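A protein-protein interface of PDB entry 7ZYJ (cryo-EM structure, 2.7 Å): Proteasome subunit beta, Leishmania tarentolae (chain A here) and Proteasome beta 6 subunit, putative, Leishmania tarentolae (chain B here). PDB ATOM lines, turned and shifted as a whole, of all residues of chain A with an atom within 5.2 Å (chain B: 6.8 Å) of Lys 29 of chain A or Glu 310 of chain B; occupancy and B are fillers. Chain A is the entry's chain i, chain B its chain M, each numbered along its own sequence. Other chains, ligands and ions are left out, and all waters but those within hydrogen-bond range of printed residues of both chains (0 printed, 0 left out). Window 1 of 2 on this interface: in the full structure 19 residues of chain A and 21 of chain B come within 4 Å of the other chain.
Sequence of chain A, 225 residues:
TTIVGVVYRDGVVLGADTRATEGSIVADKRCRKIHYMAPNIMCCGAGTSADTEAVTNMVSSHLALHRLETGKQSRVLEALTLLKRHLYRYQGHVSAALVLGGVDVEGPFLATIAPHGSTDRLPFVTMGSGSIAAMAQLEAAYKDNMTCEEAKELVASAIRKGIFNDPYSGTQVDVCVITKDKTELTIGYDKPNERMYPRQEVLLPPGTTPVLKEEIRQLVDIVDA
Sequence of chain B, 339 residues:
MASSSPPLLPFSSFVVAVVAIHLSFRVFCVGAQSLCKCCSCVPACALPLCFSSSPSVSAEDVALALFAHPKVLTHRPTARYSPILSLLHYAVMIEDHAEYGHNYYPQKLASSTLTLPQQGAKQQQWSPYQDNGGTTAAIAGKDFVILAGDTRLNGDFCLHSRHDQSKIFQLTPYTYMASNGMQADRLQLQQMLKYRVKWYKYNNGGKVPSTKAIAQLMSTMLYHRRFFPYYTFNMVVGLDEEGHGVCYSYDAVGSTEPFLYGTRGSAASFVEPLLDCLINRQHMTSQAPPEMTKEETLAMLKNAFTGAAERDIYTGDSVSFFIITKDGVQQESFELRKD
OE1 of Glu 310 of chain B lies within salt-bridge range of NZ of Lys 29 of chain A (3.99 Å).
N of Val 26 of chain A is in hydrogen-bond range of O of Arg 311 of chain B (2.8 Å).
The guanidinium group (NH1) of Arg 311 of chain B lies within hydrogen-bond range of the backbone carbonyl oxygen (O) of Ala 27 of chain A, at 2.6 Å.
Printed residues of chain A that touch a printed residue of chain B: Val 26, Ala 27, Lys 29 and Thr 171.
Hydrophobic or aromatic side chains of chain A that line the printed part of chain B: Val 26.
Lys 29 of chain A touches one residue of chain B.
Glu 310 of chain B touches two residues of chain A.
Printed residues of chain A within 4 Å of Arg 311 of chain B: Val 26 (2.8 Å) and Ala 27 (2.6 Å).
Of the printed residues of chain B, Thr 171 of chain A touches Arg 337.
Of the printed residues of chain A, Arg 337 of chain B touches Thr 171 (3.3 Å).
Printed residues of chain A within 4 Å of Ile 313 of chain B: Val 26 (3.7 Å).
The nearest printed residue of chain A that does not touch Glu 310 of chain B is Glu 194 of chain A (5.2 Å).
Glu 310 of chain B touches Val 26 of chain A (O to CB, 3.9 Å).
CG2 of Val 26 of chain A touches CG2 of Ile 313 of chain B, 3.7 Å away.
Thr 171 of chain A touches Arg 337 of chain B (CG2 to NH2, 3.3 Å).
NH1 of Arg 337 of chain B lies within salt-bridge range of OE2 of Glu 310 of chain B.
The backbone carbonyl oxygen (O) of Lys 29 of chain A sits at hydrogen-bond distance from the side-chain hydroxyl (OG1) of Thr 18 of chain A (3.2 Å).
OG1 of Thr 18 of chain A is in hydrogen-bond range of OG1 of Thr 171 of chain A, at 2.5 Å.
The backbone carbonyl oxygen (O) of Ala 20 of chain A sits at hydrogen-bond distance from the backbone NH (N) of Ala 27 of chain A, 2.8 Å away.
The backbone carbonyl oxygen (O) of Lys 29 of chain A sits at hydrogen-bond distance from the side-chain hydroxyl (OG1) of Thr 171 of chain A.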
ATOM      1  N   THR A  18     -19.441   9.767 -20.285  1.00  0.00           N
ATOM      2  CA  THR A  18     -19.328   9.394 -21.687  1.00  0.00           C
ATOM      3  C   THR A  18     -20.552   8.678 -22.240  1.00  0.00           C
ATOM      4  O   THR A  18     -20.493   8.171 -23.365  1.00  0.00           O
ATOM      5  CB  THR A  18     -18.093   8.510 -21.907  1.00  0.00           C
ATOM      6  OG1 THR A  18     -18.187   7.337 -21.090  1.00  0.00           O
ATOM      7  CG2 THR A  18     -16.825   9.268 -21.560  1.00  0.00           C
ATOM      8  N   ARG A  19     -21.653   8.618 -21.497  1.00  0.00           N
ATOM      9  CA  ARG A  19     -22.838   7.915 -21.971  1.00  0.00           C
ATOM     10  C   ARG A  19     -23.784   8.878 -22.677  1.00  0.00           C
ATOM     11  O   ARG A  19     -24.135   9.929 -22.134  1.00  0.00           O
ATOM     12  CB  ARG A  19     -23.557   7.229 -20.812  1.00  0.00           C
ATOM     13  CG  ARG A  19     -25.015   6.908 -21.107  1.00  0.00           C
ATOM     14  CD  ARG A  19     -25.717   6.324 -19.897  1.00  0.00           C
ATOM     15  NE  ARG A  19     -25.146   5.043 -19.502  1.00  0.00           N
ATOM     16  CZ  ARG A  19     -25.595   4.305 -18.497  1.00  0.00           C
ATOM     17  NH1 ARG A  19     -26.622   4.692 -17.760  1.00  0.00           N
ATOM     18  NH2 ARG A  19     -24.997   3.149 -18.224  1.00  0.00           N
ATOM     19  N   ALA A  20     -24.193   8.513 -23.890  1.00  0.00           N
ATOM     20  CA  ALA A  20     -25.197   9.248 -24.648  1.00  0.00           C
ATOM     21  C   ALA A  20     -26.418   8.355 -24.810  1.00  0.00           C
ATOM     22  O   ALA A  20     -26.305   7.235 -25.319  1.00  0.00           O
ATOM     23  CB  ALA A  20     -24.656   9.682 -26.011  1.00  0.00           C
ATOM     24  N   VAL A  26     -29.161   3.455 -24.501  1.00  0.00           N
ATOM     25  CA  VAL A  26     -27.779   3.902 -24.648  1.00  0.00           C
ATOM     26  C   VAL A  26     -27.394   3.812 -26.121  1.00  0.00           C
ATOM     27  O   VAL A  26     -27.259   2.718 -26.673  1.00  0.00           O
ATOM     28  CB  VAL A  26     -26.826   3.077 -23.777  1.00  0.00           C
ATOM     29  CG1 VAL A  26     -25.388   3.493 -24.030  1.00  0.00           C
ATOM     30  CG2 VAL A  26     -27.180   3.235 -22.308  1.00  0.00           C
ATOM     31  N   ALA A  27     -27.216   4.969 -26.761  1.00  0.00           N
ATOM     32  CA  ALA A  27     -26.779   4.995 -28.153  1.00  0.00           C
ATOM     33  C   ALA A  27     -25.282   4.735 -28.263  1.00  0.00           C
ATOM     34  O   ALA A  27     -24.852   3.771 -28.906  1.00  0.00           O
ATOM     35  CB  ALA A  27     -27.141   6.338 -28.791  1.00  0.00           C
ATOM     36  N   ASP A  28     -24.472   5.588 -27.639  1.00  0.00           N
ATOM     37  CA  ASP A  28     -23.024   5.447 -27.644  1.00  0.00           C
ATOM     38  C   ASP A  28     -22.543   5.429 -26.201  1.00  0.00           C
ATOM     39  O   ASP A  28     -23.013   6.213 -25.371  1.00  0.00           O
ATOM     40  CB  ASP A  28     -22.358   6.596 -28.424  1.00  0.00           C
ATOM     41  CG  ASP A  28     -20.837   6.504 -28.445  1.00  0.00           C
ATOM     42  OD1 ASP A  28     -20.261   5.581 -27.833  1.00  0.00           O
ATOM     43  OD2 ASP A  28     -20.210   7.373 -29.085  1.00  0.00           O
ATOM     44  N   LYS A  29     -21.604   4.534 -25.909  1.00  0.00           N
ATOM     45  CA  LYS A  29     -21.079   4.384 -24.561  1.00  0.00           C
ATOM     46  C   LYS A  29     -19.833   5.221 -24.304  1.00  0.00           C
ATOM     47  O   LYS A  29     -19.362   5.267 -23.163  1.00  0.00           O
ATOM     48  CB  LYS A  29     -20.765   2.911 -24.281  1.00  0.00           C
ATOM     49  CG  LYS A  29     -21.958   2.106 -23.796  1.00  0.00           C
ATOM     50  CD  LYS A  29     -22.062   0.782 -24.533  1.00  0.00           C
ATOM     51  CE  LYS A  29     -20.869  -0.111 -24.235  1.00  0.00           C
ATOM     52  NZ  LYS A  29     -20.798  -1.271 -25.164  1.00  0.00           N
ATOM     53  N   ARG A  30     -19.289   5.878 -25.325  1.00  0.00           N
ATOM     54  CA  ARG A  30     -18.062   6.659 -25.187  1.00  0.00           C
ATOM     55  C   ARG A  30     -18.200   7.989 -25.920  1.00  0.00           C
ATOM     56  O   ARG A  30     -17.310   8.420 -26.653  1.00  0.00           O
ATOM     57  CB  ARG A  30     -16.856   5.869 -25.690  1.00  0.00           C
ATOM     58  CG  ARG A  30     -16.474   4.702 -24.796  1.00  0.00           C
ATOM     59  CD  ARG A  30     -15.115   4.136 -25.166  1.00  0.00           C
ATOM     60  NE  ARG A  30     -14.856   2.862 -24.505  1.00  0.00           N
ATOM     61  CZ  ARG A  30     -15.423   1.711 -24.840  1.00  0.00           C
ATOM     62  NH1 ARG A  30     -16.283   1.630 -25.841  1.00  0.00           N
ATOM     63  NH2 ARG A  30     -15.117   0.613 -24.155  1.00  0.00           N
ATOM     64  N   CYS A  31     -19.339   8.652 -25.731  1.00  0.00           N
ATOM     65  CA  CYS A  31     -19.536   9.975 -26.306  1.00  0.00           C
ATOM     66  C   CYS A  31     -18.568  10.977 -25.685  1.00  0.00           C
ATOM     67  O   CYS A  31     -18.166  10.850 -24.525  1.00  0.00           O
ATOM     68  CB  CYS A  31     -20.978  10.437 -26.096  1.00  0.00           C
ATOM     69  SG  CYS A  31     -21.440  11.910 -27.037  1.00  0.00           S
ATOM     70  N   GLY A 170     -22.643   7.609 -17.276  1.00  0.00           N
ATOM     71  CA  GLY A 170     -21.782   6.510 -16.895  1.00  0.00           C
ATOM     72  C   GLY A 170     -20.760   6.172 -17.963  1.00  0.00           C
ATOM     73  O   GLY A 170     -20.524   6.932 -18.901  1.00  0.00           O
ATOM     74  N   THR A 171     -20.154   5.002 -17.769  1.00  0.00           N
ATOM     75  CA  THR A 171     -19.263   4.220 -18.622  1.00  0.00           C
ATOM     76  C   THR A 171     -17.819   4.729 -18.687  1.00  0.00           C
ATOM     77  O   THR A 171     -16.956   3.960 -19.100  1.00  0.00           O
ATOM     78  CB  THR A 171     -19.780   4.085 -20.070  1.00  0.00           C
ATOM     79  OG1 THR A 171     -19.593   5.324 -20.766  1.00  0.00           O
ATOM     80  CG2 THR A 171     -21.256   3.699 -20.100  1.00  0.00           C
ATOM     81  N   GLU A 194     -15.973  -1.752 -15.758  1.00  0.00           N
ATOM     82  CA  GLU A 194     -15.132  -2.503 -16.675  1.00  0.00           C
ATOM     83  C   GLU A 194     -15.974  -3.496 -17.475  1.00  0.00           C
ATOM     84  O   GLU A 194     -17.204  -3.535 -17.380  1.00  0.00           O
ATOM     85  CB  GLU A 194     -14.020  -3.215 -15.909  1.00  0.00           C
ATOM     86  CG  GLU A 194     -13.042  -2.276 -15.224  1.00  0.00           C
ATOM     87  CD  GLU A 194     -12.008  -3.016 -14.401  1.00  0.00           C
ATOM     88  OE1 GLU A 194     -12.139  -4.248 -14.247  1.00  0.00           O
ATOM     89  OE2 GLU A 194     -11.063  -2.365 -13.907  1.00  0.00           O
ATOM     90  N   PHE B 305     -28.954 -10.910 -20.341  1.00  0.00           N
ATOM     91  CA  PHE B 305     -28.997  -9.858 -19.328  1.00  0.00           C
ATOM     92  C   PHE B 305     -27.764  -8.963 -19.385  1.00  0.00           C
ATOM     93  O   PHE B 305     -27.870  -7.749 -19.181  1.00  0.00           O
ATOM     94  CB  PHE B 305     -29.169 -10.462 -17.935  1.00  0.00           C
ATOM     95  CG  PHE B 305     -30.579 -10.871 -17.628  1.00  0.00           C
ATOM     96  CD1 PHE B 305     -31.500  -9.931 -17.197  1.00  0.00           C
ATOM     97  CD2 PHE B 305     -30.990 -12.181 -17.780  1.00  0.00           C
ATOM     98  CE1 PHE B 305     -32.801 -10.292 -16.915  1.00  0.00           C
ATOM     99  CE2 PHE B 305     -32.290 -12.546 -17.503  1.00  0.00           C
ATOM    100  CZ  PHE B 305     -33.196 -11.602 -17.068  1.00  0.00           C
ATOM    101  N   THR B 306     -26.586  -9.535 -19.652  1.00  0.00           N
ATOM    102  CA  THR B 306     -25.384  -8.716 -19.764  1.00  0.00           C
ATOM    103  C   THR B 306     -25.500  -7.731 -20.919  1.00  0.00           C
ATOM    104  O   THR B 306     -25.145  -6.555 -20.782  1.00  0.00           O
ATOM    105  CB  THR B 306     -24.153  -9.604 -19.937  1.00  0.00           C
ATOM    106  OG1 THR B 306     -23.985 -10.425 -18.774  1.00  0.00           O
ATOM    107  CG2 THR B 306     -22.906  -8.757 -20.130  1.00  0.00           C
ATOM    108  N   GLY B 307     -26.007  -8.191 -22.065  1.00  0.00           N
ATOM    109  CA  GLY B 307     -26.225  -7.291 -23.183  1.00  0.00           C
ATOM    110  C   GLY B 307     -27.283  -6.244 -22.906  1.00  0.00           C
ATOM    111  O   GLY B 307     -27.139  -5.090 -23.319  1.00  0.00           O
ATOM    112  N   ALA B 308     -28.358  -6.626 -22.214  1.00  0.00           N
ATOM    113  CA  ALA B 308     -29.409  -5.666 -21.889  1.00  0.00           C
ATOM    114  C   ALA B 308     -28.904  -4.582 -20.944  1.00  0.00           C
ATOM    115  O   ALA B 308     -29.245  -3.405 -21.103  1.00  0.00           O
ATOM    116  CB  ALA B 308     -30.609  -6.390 -21.281  1.00  0.00           C
ATOM    117  N   ALA B 309     -28.094  -4.959 -19.953  1.00  0.00           N
ATOM    118  CA  ALA B 309     -27.619  -4.005 -18.959  1.00  0.00           C
ATOM    119  C   ALA B 309     -26.672  -2.961 -19.536  1.00  0.00           C
ATOM    120  O   ALA B 309     -26.487  -1.912 -18.911  1.00  0.00           O
ATOM    121  CB  ALA B 309     -26.930  -4.746 -17.812  1.00  0.00           C
ATOM    122  N   GLU B 310     -26.073  -3.214 -20.698  1.00  0.00           N
ATOM    123  CA  GLU B 310     -25.162  -2.263 -21.318  1.00  0.00           C
ATOM    124  C   GLU B 310     -25.856  -1.288 -22.259  1.00  0.00           C
ATOM    125  O   GLU B 310     -25.211  -0.345 -22.730  1.00  0.00           O
ATOM    126  CB  GLU B 310     -24.057  -3.005 -22.081  1.00  0.00           C
ATOM    127  CG  GLU B 310     -23.285  -4.003 -21.238  1.00  0.00           C
ATOM    128  CD  GLU B 310     -21.868  -4.212 -21.730  1.00  0.00           C
ATOM    129  OE1 GLU B 310     -21.687  -4.461 -22.941  1.00  0.00           O
ATOM    130  OE2 GLU B 310     -20.933  -4.127 -20.908  1.00  0.00           O
ATOM    131  N   ARG B 311     -27.141  -1.487 -22.545  1.00  0.00           N
ATOM    132  CA  ARG B 311     -27.875  -0.602 -23.442  1.00  0.00           C
ATOM    133  C   ARG B 311     -29.151  -0.029 -22.846  1.00  0.00           C
ATOM    134  O   ARG B 311     -29.628   0.997 -23.343  1.00  0.00           O
ATOM    135  CB  ARG B 311     -28.225  -1.330 -24.748  1.00  0.00           C
ATOM    136  CG  ARG B 311     -27.014  -1.686 -25.596  1.00  0.00           C
ATOM    137  CD  ARG B 311     -26.563  -0.505 -26.437  1.00  0.00           C
ATOM    138  NE  ARG B 311     -25.256  -0.732 -27.039  1.00  0.00           N
ATOM    139  CZ  ARG B 311     -24.578   0.178 -27.723  1.00  0.00           C
ATOM    140  NH1 ARG B 311     -25.058   1.396 -27.917  1.00  0.00           N
ATOM    141  NH2 ARG B 311     -23.388  -0.140 -28.224  1.00  0.00           N
ATOM    142  N   ASP B 312     -29.719  -0.644 -21.813  1.00  0.00           N
ATOM    143  CA  ASP B 312     -30.916  -0.138 -21.159  1.00  0.00           C
ATOM    144  C   ASP B 312     -30.527   0.505 -19.835  1.00  0.00           C
ATOM    145  O   ASP B 312     -29.861  -0.124 -19.005  1.00  0.00           O
ATOM    146  CB  ASP B 312     -31.930  -1.260 -20.934  1.00  0.00           C
ATOM    147  CG  ASP B 312     -33.291  -0.741 -20.525  1.00  0.00           C
ATOM    148  OD1 ASP B 312     -33.682   0.348 -20.995  1.00  0.00           O
ATOM    149  OD2 ASP B 312     -33.972  -1.422 -19.731  1.00  0.00           O
ATOM    150  N   ILE B 313     -30.944   1.760 -19.641  1.00  0.00           N
ATOM    151  CA  ILE B 313     -30.489   2.535 -18.488  1.00  0.00           C
ATOM    152  C   ILE B 313     -31.259   2.239 -17.212  1.00  0.00           C
ATOM    153  O   ILE B 313     -30.800   2.616 -16.127  1.00  0.00           O
ATOM    154  CB  ILE B 313     -30.577   4.045 -18.777  1.00  0.00           C
ATOM    155  CG1 ILE B 313     -32.033   4.508 -18.772  1.00  0.00           C
ATOM    156  CG2 ILE B 313     -29.923   4.369 -20.110  1.00  0.00           C
ATOM    157  CD1 ILE B 313     -32.192   6.010 -18.785  1.00  0.00           C
ATOM    158  N   THR B 315     -32.217  -0.892 -16.114  1.00  0.00           N
ATOM    159  CA  THR B 315     -32.025  -2.246 -15.623  1.00  0.00           C
ATOM    160  C   THR B 315     -30.548  -2.529 -15.390  1.00  0.00           C
ATOM    161  O   THR B 315     -29.675  -2.009 -16.093  1.00  0.00           O
ATOM    162  CB  THR B 315     -32.601  -3.288 -16.595  1.00  0.00           C
ATOM    163  OG1 THR B 315     -32.450  -4.598 -16.035  1.00  0.00           O
ATOM    164  CG2 THR B 315     -31.888  -3.235 -17.933  1.00  0.00           C
ATOM    165  N   ARG B 337     -23.361  -4.534 -14.307  1.00  0.00           N
ATOM    166  CA  ARG B 337     -22.817  -3.196 -14.140  1.00  0.00           C
ATOM    167  C   ARG B 337     -23.705  -2.373 -13.213  1.00  0.00           C
ATOM    168  O   ARG B 337     -24.906  -2.615 -13.093  1.00  0.00           O
ATOM    169  CB  ARG B 337     -22.690  -2.510 -15.497  1.00  0.00           C
ATOM    170  CG  ARG B 337     -21.668  -3.149 -16.417  1.00  0.00           C
ATOM    171  CD  ARG B 337     -21.617  -2.433 -17.751  1.00  0.00           C
ATOM    172  NE  ARG B 337     -21.109  -1.074 -17.616  1.00  0.00           N
ATOM    173  CZ  ARG B 337     -21.109  -0.175 -18.590  1.00  0.00           C
ATOM    174  NH1 ARG B 337     -21.594  -0.455 -19.788  1.00  0.00           N
ATOM    175  NH2 ARG B 337     -20.611   1.034 -18.355  1.00  0.00           N
